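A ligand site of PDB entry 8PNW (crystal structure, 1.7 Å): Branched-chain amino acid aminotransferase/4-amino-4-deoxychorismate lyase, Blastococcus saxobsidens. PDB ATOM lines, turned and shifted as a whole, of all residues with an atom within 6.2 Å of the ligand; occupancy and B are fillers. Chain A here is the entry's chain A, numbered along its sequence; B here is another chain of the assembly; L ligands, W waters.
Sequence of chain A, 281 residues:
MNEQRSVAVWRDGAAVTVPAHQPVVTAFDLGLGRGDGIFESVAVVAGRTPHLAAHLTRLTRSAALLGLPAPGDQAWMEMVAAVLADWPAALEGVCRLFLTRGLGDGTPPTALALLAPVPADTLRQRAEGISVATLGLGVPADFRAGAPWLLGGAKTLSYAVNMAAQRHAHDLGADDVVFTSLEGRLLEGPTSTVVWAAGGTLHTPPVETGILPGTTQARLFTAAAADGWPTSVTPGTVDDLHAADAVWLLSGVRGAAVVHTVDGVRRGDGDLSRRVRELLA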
ATOM      1  N   PHE A  39     -20.589  -4.748   7.591  1.00  0.00           N
ATOM      2  CA  PHE A  39     -19.553  -5.672   7.092  1.00  0.00           C
ATOM      3  C   PHE A  39     -18.425  -5.832   8.116  1.00  0.00           C
ATOM      4  O   PHE A  39     -18.253  -5.033   9.025  1.00  0.00           O
ATOM      5  CB  PHE A  39     -19.003  -5.244   5.729  1.00  0.00           C
ATOM      6  CG  PHE A  39     -17.997  -4.151   5.774  1.00  0.00           C
ATOM      7  CD1 PHE A  39     -18.378  -2.843   6.021  1.00  0.00           C
ATOM      8  CD2 PHE A  39     -16.643  -4.410   5.539  1.00  0.00           C
ATOM      9  CE1 PHE A  39     -17.451  -1.824   6.072  1.00  0.00           C
ATOM     10  CE2 PHE A  39     -15.723  -3.375   5.552  1.00  0.00           C
ATOM     11  CZ  PHE A  39     -16.120  -2.087   5.832  1.00  0.00           C
ATOM     12  N   GLU A  40     -17.634  -6.863   7.861  1.00  0.00           N
ATOM     13  CA  GLU A  40     -16.315  -7.084   8.457  1.00  0.00           C
ATOM     14  C   GLU A  40     -15.300  -7.421   7.353  1.00  0.00           C
ATOM     15  O   GLU A  40     -15.668  -7.986   6.319  1.00  0.00           O
ATOM     16  CB  GLU A  40     -16.412  -8.211   9.485  1.00  0.00           C
ATOM     17  CG  GLU A  40     -16.976  -7.727  10.801  1.00  0.00           C
ATOM     18  CD  GLU A  40     -16.101  -6.727  11.506  1.00  0.00           C
ATOM     19  OE1 GLU A  40     -14.851  -6.733  11.282  1.00  0.00           O
ATOM     20  OE2 GLU A  40     -16.669  -5.931  12.247  1.00  0.00           O
ATOM     21  N   SER A  41     -14.063  -7.046   7.579  1.00  0.00           N
ATOM     22  CA  SER A  41     -12.932  -7.317   6.679  1.00  0.00           C
ATOM     23  C   SER A  41     -11.940  -8.205   7.418  1.00  0.00           C
ATOM     24  O   SER A  41     -11.279  -7.707   8.332  1.00  0.00           O
ATOM     25  CB  SER A  41     -12.351  -6.000   6.247  1.00  0.00           C
ATOM     26  OG  SER A  41     -11.297  -6.174   5.341  1.00  0.00           O
ATOM     27  N   HIS A  55     -13.552 -10.237  14.776  1.00  0.00           N
ATOM     28  CA  HIS A  55     -14.432  -9.644  13.734  1.00  0.00           C
ATOM     29  C   HIS A  55     -15.891 -10.082  13.962  1.00  0.00           C
ATOM     30  O   HIS A  55     -16.834  -9.256  13.801  1.00  0.00           O
ATOM     31  CB  HIS A  55     -13.962  -9.984  12.333  1.00  0.00           C
ATOM     32  CG  HIS A  55     -12.615  -9.439  12.043  1.00  0.00           C
ATOM     33  ND1 HIS A  55     -12.447  -8.126  11.692  1.00  0.00           N
ATOM     34  CD2 HIS A  55     -11.378  -9.955  12.115  1.00  0.00           C
ATOM     35  CE1 HIS A  55     -11.164  -7.874  11.498  1.00  0.00           C
ATOM     36  NE2 HIS A  55     -10.476  -8.973  11.772  1.00  0.00           N
ATOM     37  N   ARG A  58     -17.513  -8.046  16.757  1.00  0.00           N
ATOM     38  CA  ARG A  58     -17.847  -6.672  16.322  1.00  0.00           C
ATOM     39  C   ARG A  58     -19.007  -6.746  15.303  1.00  0.00           C
ATOM     40  O   ARG A  58     -19.830  -5.830  15.310  1.00  0.00           O
ATOM     41  CB  ARG A  58     -16.632  -5.970  15.713  1.00  0.00           C
ATOM     42  CG  ARG A  58     -16.930  -4.507  15.403  1.00  0.00           C
ATOM     43  CD  ARG A  58     -15.699  -3.705  15.051  1.00  0.00           C
ATOM     44  NE  ARG A  58     -15.136  -4.175  13.786  1.00  0.00           N
ATOM     45  CZ  ARG A  58     -13.900  -3.888  13.366  1.00  0.00           C
ATOM     46  NH1 ARG A  58     -13.130  -3.075  14.068  1.00  0.00           N
ATOM     47  NH2 ARG A  58     -13.424  -4.445  12.285  1.00  0.00           N
ATOM     48  N   LYS A 155     -19.664  -0.560  11.544  1.00  0.00           N
ATOM     49  CA  LYS A 155     -18.866  -0.795  10.314  1.00  0.00           C
ATOM     50  C   LYS A 155     -19.900  -1.067   9.219  1.00  0.00           C
ATOM     51  O   LYS A 155     -20.382  -2.180   9.142  1.00  0.00           O
ATOM     52  CB  LYS A 155     -17.868  -1.924  10.515  1.00  0.00           C
ATOM     53  CG  LYS A 155     -16.726  -2.004   9.503  1.00  0.00           C
ATOM     54  CD  LYS A 155     -15.621  -3.003   9.926  1.00  0.00           C
ATOM     55  CE  LYS A 155     -14.394  -3.067   9.038  1.00  0.00           C
ATOM     56  NZ  LYS A 155     -13.724  -1.772   8.905  1.00  0.00           N
ATOM     57  N   THR A 156     -20.261  -0.043   8.424  1.00  0.00           N
ATOM     58  CA  THR A 156     -21.451  -0.151   7.532  1.00  0.00           C
ATOM     59  C   THR A 156     -21.058  -0.222   6.058  1.00  0.00           C
ATOM     60  O   THR A 156     -19.915   0.115   5.685  1.00  0.00           O
ATOM     61  CB  THR A 156     -22.435   0.994   7.741  1.00  0.00           C
ATOM     62  OG1 THR A 156     -21.910   2.142   7.072  1.00  0.00           O
ATOM     63  CG2 THR A 156     -22.652   1.289   9.213  1.00  0.00           C
ATOM     64  N   TYR A 159     -20.309   3.698   2.828  1.00  0.00           N
ATOM     65  CA  TYR A 159     -18.950   4.277   2.923  1.00  0.00           C
ATOM     66  C   TYR A 159     -18.634   5.138   1.690  1.00  0.00           C
ATOM     67  O   TYR A 159     -17.442   5.354   1.331  1.00  0.00           O
ATOM     68  CB  TYR A 159     -17.930   3.148   3.100  1.00  0.00           C
ATOM     69  CG  TYR A 159     -17.566   2.790   4.515  1.00  0.00           C
ATOM     70  CD1 TYR A 159     -18.425   3.043   5.582  1.00  0.00           C
ATOM     71  CD2 TYR A 159     -16.319   2.238   4.776  1.00  0.00           C
ATOM     72  CE1 TYR A 159     -18.088   2.663   6.881  1.00  0.00           C
ATOM     73  CE2 TYR A 159     -15.965   1.874   6.065  1.00  0.00           C
ATOM     74  CZ  TYR A 159     -16.876   2.037   7.098  1.00  0.00           C
ATOM     75  OH  TYR A 159     -16.520   1.686   8.370  1.00  0.00           O
ATOM     76  N   ASN A 162     -16.325   7.802   2.960  1.00  0.00           N
ATOM     77  CA  ASN A 162     -15.029   7.128   3.234  1.00  0.00           C
ATOM     78  C   ASN A 162     -14.208   7.021   1.958  1.00  0.00           C
ATOM     79  O   ASN A 162     -13.054   7.467   1.935  1.00  0.00           O
ATOM     80  CB  ASN A 162     -15.290   5.782   3.869  1.00  0.00           C
ATOM     81  CG  ASN A 162     -16.149   5.910   5.111  1.00  0.00           C
ATOM     82  OD1 ASN A 162     -17.319   6.333   5.025  1.00  0.00           O
ATOM     83  ND2 ASN A 162     -15.610   5.474   6.233  1.00  0.00           N
ATOM     84  N   GLU A 188     -10.206   8.906  13.024  1.00  0.00           N
ATOM     85  CA  GLU A 188      -9.735   7.623  12.487  1.00  0.00           C
ATOM     86  C   GLU A 188      -9.566   7.764  10.997  1.00  0.00           C
ATOM     87  O   GLU A 188      -9.931   8.840  10.429  1.00  0.00           O
ATOM     88  CB  GLU A 188     -10.700   6.481  12.828  1.00  0.00           C
ATOM     89  CG  GLU A 188     -12.085   6.632  12.194  1.00  0.00           C
ATOM     90  CD  GLU A 188     -13.099   5.589  12.641  1.00  0.00           C
ATOM     91  OE1 GLU A 188     -12.680   4.425  12.914  1.00  0.00           O
ATOM     92  OE2 GLU A 188     -14.318   5.946  12.680  1.00  0.00           O
ATOM     93  N   GLY A 189      -9.033   6.717  10.373  1.00  0.00           N
ATOM     94  CA  GLY A 189      -8.993   6.641   8.894  1.00  0.00           C
ATOM     95  C   GLY A 189     -10.345   6.198   8.364  1.00  0.00           C
ATOM     96  O   GLY A 189     -11.214   5.721   9.110  1.00  0.00           O
ATOM     97  N   PRO A 190     -10.574   6.346   7.041  1.00  0.00           N
ATOM     98  CA  PRO A 190     -11.789   5.858   6.390  1.00  0.00           C
ATOM     99  C   PRO A 190     -11.982   4.350   6.619  1.00  0.00           C
ATOM    100  O   PRO A 190     -13.114   3.922   6.646  1.00  0.00           O
ATOM    101  CB  PRO A 190     -11.547   6.138   4.894  1.00  0.00           C
ATOM    102  CG  PRO A 190     -10.489   7.186   4.846  1.00  0.00           C
ATOM    103  CD  PRO A 190      -9.632   6.955   6.088  1.00  0.00           C
ATOM    104  N   THR A 191     -10.895   3.596   6.723  1.00  0.00           N
ATOM    105  CA  THR A 191     -10.960   2.103   6.872  1.00  0.00           C
ATOM    106  C   THR A 191      -9.909   1.624   7.879  1.00  0.00           C
ATOM    107  O   THR A 191      -9.544   0.433   7.821  1.00  0.00           O
ATOM    108  CB  THR A 191     -10.759   1.382   5.530  1.00  0.00           C
ATOM    109  OG1 THR A 191      -9.440   1.638   5.041  1.00  0.00           O
ATOM    110  CG2 THR A 191     -11.818   1.708   4.497  1.00  0.00           C
ATOM    111  N   SER A 192      -9.425   2.482   8.763  1.00  0.00           N
ATOM    112  CA  SER A 192      -8.274   2.145   9.627  1.00  0.00           C
ATOM    113  C   SER A 192      -8.265   3.026  10.855  1.00  0.00           C
ATOM    114  O   SER A 192      -9.033   3.998  10.923  1.00  0.00           O
ATOM    115  CB  SER A 192      -6.971   2.261   8.849  1.00  0.00           C
ATOM    116  OG  SER A 192      -6.796   3.587   8.339  1.00  0.00           O
ATOM    117  N   THR A 193      -7.452   2.623  11.810  1.00  0.00           N
ATOM    118  CA  THR A 193      -7.331   3.243  13.142  1.00  0.00           C
ATOM    119  C   THR A 193      -5.975   3.914  13.300  1.00  0.00           C
ATOM    120  O   THR A 193      -4.970   3.362  12.832  1.00  0.00           O
ATOM    121  CB  THR A 193      -7.438   2.133  14.201  1.00  0.00           C
ATOM    122  OG1 THR A 193      -8.682   1.484  13.977  1.00  0.00           O
ATOM    123  CG2 THR A 193      -7.374   2.709  15.595  1.00  0.00           C
ATOM    124  N   LEU A 212     -14.916   3.814  15.041  1.00  0.00           N
ATOM    125  CA  LEU A 212     -15.038   2.345  15.140  1.00  0.00           C
ATOM    126  C   LEU A 212     -13.985   1.874  16.152  1.00  0.00           C
ATOM    127  O   LEU A 212     -12.831   2.290  16.048  1.00  0.00           O
ATOM    128  CB  LEU A 212     -14.806   1.691  13.781  1.00  0.00           C
ATOM    129  CG  LEU A 212     -15.292   0.260  13.680  1.00  0.00           C
ATOM    130  CD1 LEU A 212     -16.820   0.195  13.776  1.00  0.00           C
ATOM    131  CD2 LEU A 212     -14.790  -0.401  12.387  1.00  0.00           C
ATOM    132  N   PRO A 213     -14.299   0.984  17.109  1.00  0.00           N
ATOM    133  CA  PRO A 213     -13.251   0.367  17.906  1.00  0.00           C
ATOM    134  C   PRO A 213     -12.484  -0.625  17.027  1.00  0.00           C
ATOM    135  O   PRO A 213     -13.060  -1.616  16.583  1.00  0.00           O
ATOM    136  CB  PRO A 213     -13.960  -0.364  19.043  1.00  0.00           C
ATOM    137  CG  PRO A 213     -15.417  -0.023  18.882  1.00  0.00           C
ATOM    138  CD  PRO A 213     -15.644   0.521  17.495  1.00  0.00           C
ATOM    139  N   GLY A 214     -11.230  -0.316  16.728  1.00  0.00           N
ATOM    140  CA  GLY A 214     -10.431  -1.135  15.808  1.00  0.00           C
ATOM    141  C   GLY A 214      -9.885  -2.377  16.481  1.00  0.00           C
ATOM    142  O   GLY A 214      -9.236  -2.245  17.544  1.00  0.00           O
ATOM    143  N   THR A 215     -10.025  -3.525  15.824  1.00  0.00           N
ATOM    144  CA  THR A 215      -9.539  -4.820  16.399  1.00  0.00           C
ATOM    145  C   THR A 215      -8.010  -4.896  16.325  1.00  0.00           C
ATOM    146  O   THR A 215      -7.379  -5.476  17.253  1.00  0.00           O
ATOM    147  CB  THR A 215     -10.223  -6.020  15.739  1.00  0.00           C
ATOM    148  OG1 THR A 215      -9.845  -6.209  14.384  1.00  0.00           O
ATOM    149  CG2 THR A 215     -11.730  -5.897  15.898  1.00  0.00           C
ATOM    150  N   THR A 216      -7.405  -4.358  15.262  1.00  0.00           N
ATOM    151  CA  THR A 216      -5.947  -4.408  15.105  1.00  0.00           C
ATOM    152  C   THR A 216      -5.272  -3.540  16.179  1.00  0.00           C
ATOM    153  O   THR A 216      -4.330  -4.011  16.787  1.00  0.00           O
ATOM    154  CB  THR A 216      -5.527  -4.047  13.683  1.00  0.00           C
ATOM    155  OG1 THR A 216      -6.300  -4.759  12.719  1.00  0.00           O
ATOM    156  CG2 THR A 216      -4.058  -4.286  13.490  1.00  0.00           C
ATOM    157  N   GLN A 217      -5.767  -2.317  16.371  1.00  0.00           N
ATOM    158  CA  GLN A 217      -5.315  -1.422  17.441  1.00  0.00           C
ATOM    159  C   GLN A 217      -5.463  -2.128  18.788  1.00  0.00           C
ATOM    160  O   GLN A 217      -4.496  -2.084  19.560  1.00  0.00           O
ATOM    161  CB  GLN A 217      -6.051  -0.100  17.378  1.00  0.00           C
ATOM    162  CG  GLN A 217      -5.735   0.795  18.560  1.00  0.00           C
ATOM    163  CD  GLN A 217      -6.648   0.572  19.734  1.00  0.00           C
ATOM    164  OE1 GLN A 217      -7.857   0.619  19.608  1.00  0.00           O
ATOM    165  NE2 GLN A 217      -6.065   0.399  20.912  1.00  0.00           N
ATOM    166  N   LEU A 250      -3.654   1.365  11.300  1.00  0.00           N
ATOM    167  CA  LEU A 250      -3.849  -0.085  11.537  1.00  0.00           C
ATOM    168  C   LEU A 250      -5.221  -0.516  11.013  1.00  0.00           C
ATOM    169  O   LEU A 250      -6.243   0.172  11.295  1.00  0.00           O
ATOM    170  CB  LEU A 250      -3.740  -0.434  13.020  1.00  0.00           C
ATOM    171  CG  LEU A 250      -2.515   0.066  13.773  1.00  0.00           C
ATOM    172  CD1 LEU A 250      -2.546  -0.407  15.212  1.00  0.00           C
ATOM    173  CD2 LEU A 250      -1.218  -0.363  13.147  1.00  0.00           C
ATOM    174  N   SER A 251      -5.244  -1.695  10.396  1.00  0.00           N
ATOM    175  CA  SER A 251      -6.473  -2.355   9.903  1.00  0.00           C
ATOM    176  C   SER A 251      -6.259  -3.852   9.710  1.00  0.00           C
ATOM    177  O   SER A 251      -5.089  -4.290   9.643  1.00  0.00           O
ATOM    178  CB  SER A 251      -6.924  -1.683   8.652  1.00  0.00           C
ATOM    179  OG  SER A 251      -5.901  -1.796   7.688  1.00  0.00           O
ATOM    180  N   GLY A 252      -7.360  -4.601   9.720  1.00  0.00           N
ATOM    181  CA  GLY A 252      -7.324  -6.068   9.629  1.00  0.00           C
ATOM    182  C   GLY A 252      -6.572  -6.566   8.414  1.00  0.00           C
ATOM    183  O   GLY A 252      -5.817  -7.527   8.543  1.00  0.00           O
ATOM    184  N   VAL A 253      -6.776  -5.973   7.265  1.00  0.00           N
ATOM    185  CA  VAL A 253      -6.190  -6.519   6.011  1.00  0.00           C
ATOM    186  C   VAL A 253      -4.850  -5.844   5.734  1.00  0.00           C
ATOM    187  O   VAL A 253      -3.829  -6.563   5.720  1.00  0.00           O
ATOM    188  CB  VAL A 253      -7.216  -6.438   4.856  1.00  0.00           C
ATOM    189  CG1 VAL A 253      -6.518  -6.747   3.533  1.00  0.00           C
ATOM    190  CG2 VAL A 253      -8.365  -7.417   5.133  1.00  0.00           C
ATOM    191  N   ARG B  34     -19.521  -0.769  -0.693  1.00  0.00           N
ATOM    192  CA  ARG B  34     -19.130   0.562  -0.178  1.00  0.00           C
ATOM    193  C   ARG B  34     -20.263   1.573  -0.311  1.00  0.00           C
ATOM    194  O   ARG B  34     -20.087   2.688   0.119  1.00  0.00           O
ATOM    195  CB  ARG B  34     -17.932   1.076  -0.991  1.00  0.00           C
ATOM    196  CG  ARG B  34     -16.653   0.262  -0.811  1.00  0.00           C
ATOM    197  CD  ARG B  34     -16.179   0.300   0.612  1.00  0.00           C
ATOM    198  NE  ARG B  34     -14.801  -0.210   0.756  1.00  0.00           N
ATOM    199  CZ  ARG B  34     -14.249  -0.590   1.918  1.00  0.00           C
ATOM    200  NH1 ARG B  34     -14.940  -0.603   3.042  1.00  0.00           N
ATOM    201  NH2 ARG B  34     -12.985  -0.984   1.952  1.00  0.00           N
HETATM  202  N1  LIG L   1     -11.962   2.372  11.054  1.00  0.00           N
HETATM  203  C1  LIG L   1     -12.931   2.158  10.170  1.00  0.00           C
HETATM  204  C2  LIG L   1     -13.841   3.294   9.845  1.00  0.00           C
HETATM  205  C3  LIG L   1     -13.117   0.873   9.631  1.00  0.00           C
HETATM  206  O1  LIG L   1     -14.142   0.690   8.774  1.00  0.00           O
HETATM  207  C4  LIG L   1     -12.271  -0.203   9.997  1.00  0.00           C
HETATM  208  C5  LIG L   1     -12.607  -1.526   9.558  1.00  0.00           C
HETATM  209  C6  LIG L   1     -11.208   0.101  10.865  1.00  0.00           C
HETATM  210  C7  LIG L   1     -11.105   1.363  11.357  1.00  0.00           C
HETATM  211  C8  LIG L   1     -10.161  -0.905  11.228  1.00  0.00           C
HETATM  212  O2  LIG L   1     -10.589  -1.951  12.141  1.00  0.00           O
HETATM  213  P1  LIG L   1      -9.825  -3.392  12.119  1.00  0.00           P
HETATM  214  O3  LIG L   1      -9.853  -3.872  10.702  1.00  0.00           O
HETATM  215  O4  LIG L   1      -8.441  -3.147  12.706  1.00  0.00           O
HETATM  216  O5  LIG L   1     -10.743  -4.195  13.038  1.00  0.00           O
HETATM  217  O   HOH W   1     -11.850  -5.405   9.625  1.00  0.00           O
HETATM  218  O   HOH W   2     -10.575  -2.014   7.266  1.00  0.00           O
HETATM  219  O   HOH W   3      -7.526  -1.208  14.322  1.00  0.00           O
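The backbone carbonyl oxygen of Lys 155 is in hydrogen-bond range of the backbone NH of Phe 39, 3.0 Å away.
The backbone carbonyl oxygen of Arg 34 of chain B is in hydrogen-bond range of the backbone NH of Tyr 159, at 2.9 Å.
N of Gly 252 sits at hydrogen-bond distance from OG1 of Thr 216 (3.2 Å).
The side-chain hydroxyl (OG1) of Thr 216 lies close to the backbone carbonyl oxygen (O) of Ser 251, 3.3 Å away.
NH1 of Arg 58 sits at hydrogen-bond distance from O of Pro 213 (2.9 Å).
The guanidinium group (NE) of Arg 58 is in salt-bridge range of the side-chain carboxylate (OE2) of Glu 40, 2.8 Å away.
The side-chain amide nitrogen (ND2) of Asn 162 sits at hydrogen-bond distance from the backbone carbonyl oxygen (O) of Pro 190 (3.0 Å).
The backbone carbonyl oxygen (O) of Leu 250 is in hydrogen-bond range of the backbone NH (N) of Thr 193, 2.8 Å away.
Water W3 lies within hydrogen-bond range of O4 of the ligand (2.7 Å), N of Gln 217 (2.9 Å), OG1 of Thr 193 (2.9 Å) and N of Thr 216 (3.3 Å).
Water W1 lies within hydrogen-bond range of O of Ser 41, O3 of the ligand, NH2 of Arg 58 and ND1 of His 55.
C5 of the ligand is covalently linked to NZ of Lys 155, 1.3 Å away.
N of Thr 215 lies within hydrogen-bond range of O5 of the ligand, 3.0 Å away.
An oxygen (O5) of the ligand lies within hydrogen-bond range of the side-chain hydroxyl of Thr 215, at 2.6 Å.
The side-chain hydroxyl (OH) of Tyr 159 is in hydrogen-bond range of an oxygen (O1) of the ligand (2.6 Å).
O4 of the ligand lies within hydrogen-bond range of N of Thr 216.
The side-chain hydroxyl (OG1) of Thr 216 sits at hydrogen-bond distance from an oxygen (O4) of the ligand.
An oxygen (O3) of the ligand sits at hydrogen-bond distance from the backbone NH (N) of Gly 252, 2.8 Å away.
The guanidinium group (NH2) of Arg 58 lies within salt-bridge range of an oxygen (O5) of the ligand, at 2.8 Å.
The side-chain carboxylate (OE1) of Glu 188 sits at hydrogen-bond distance from a nitrogen (N1) of the ligand.
N of Ser 192 lies close to N1 of the ligand, at 3.4 Å.
O of Gly 189 touches C2 of the ligand, 3.7 Å away.
Pro 190 touches the ligand (O to C2, 3.3 Å).
O of Thr 191 touches C6 of the ligand (3.5 Å).
Thr 193 touches the ligand (OG1 to C7, 3.6 Å).
CD2 of Leu 212 touches C3 of the ligand, at 3.5 Å.
Gly 214 touches the ligand.
CA of Ser 251 touches O4 of the ligand, at 3.5 Å.
Hydrophobic or aromatic side chains within 4 Å of the ligand: Tyr 159 and Leu 212.
15 residues have an atom within 4 Å of the ligand: Arg 58, Lys 155, Tyr 159, Glu 188, Gly 189, Pro 190, Thr 191, Ser 192, Thr 193, Leu 212, Gly 214, Thr 215, Thr 216, Ser 251 and Gly 252.
The nearest printed residue that does not touch the ligand is His 55 (4.01 Å).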
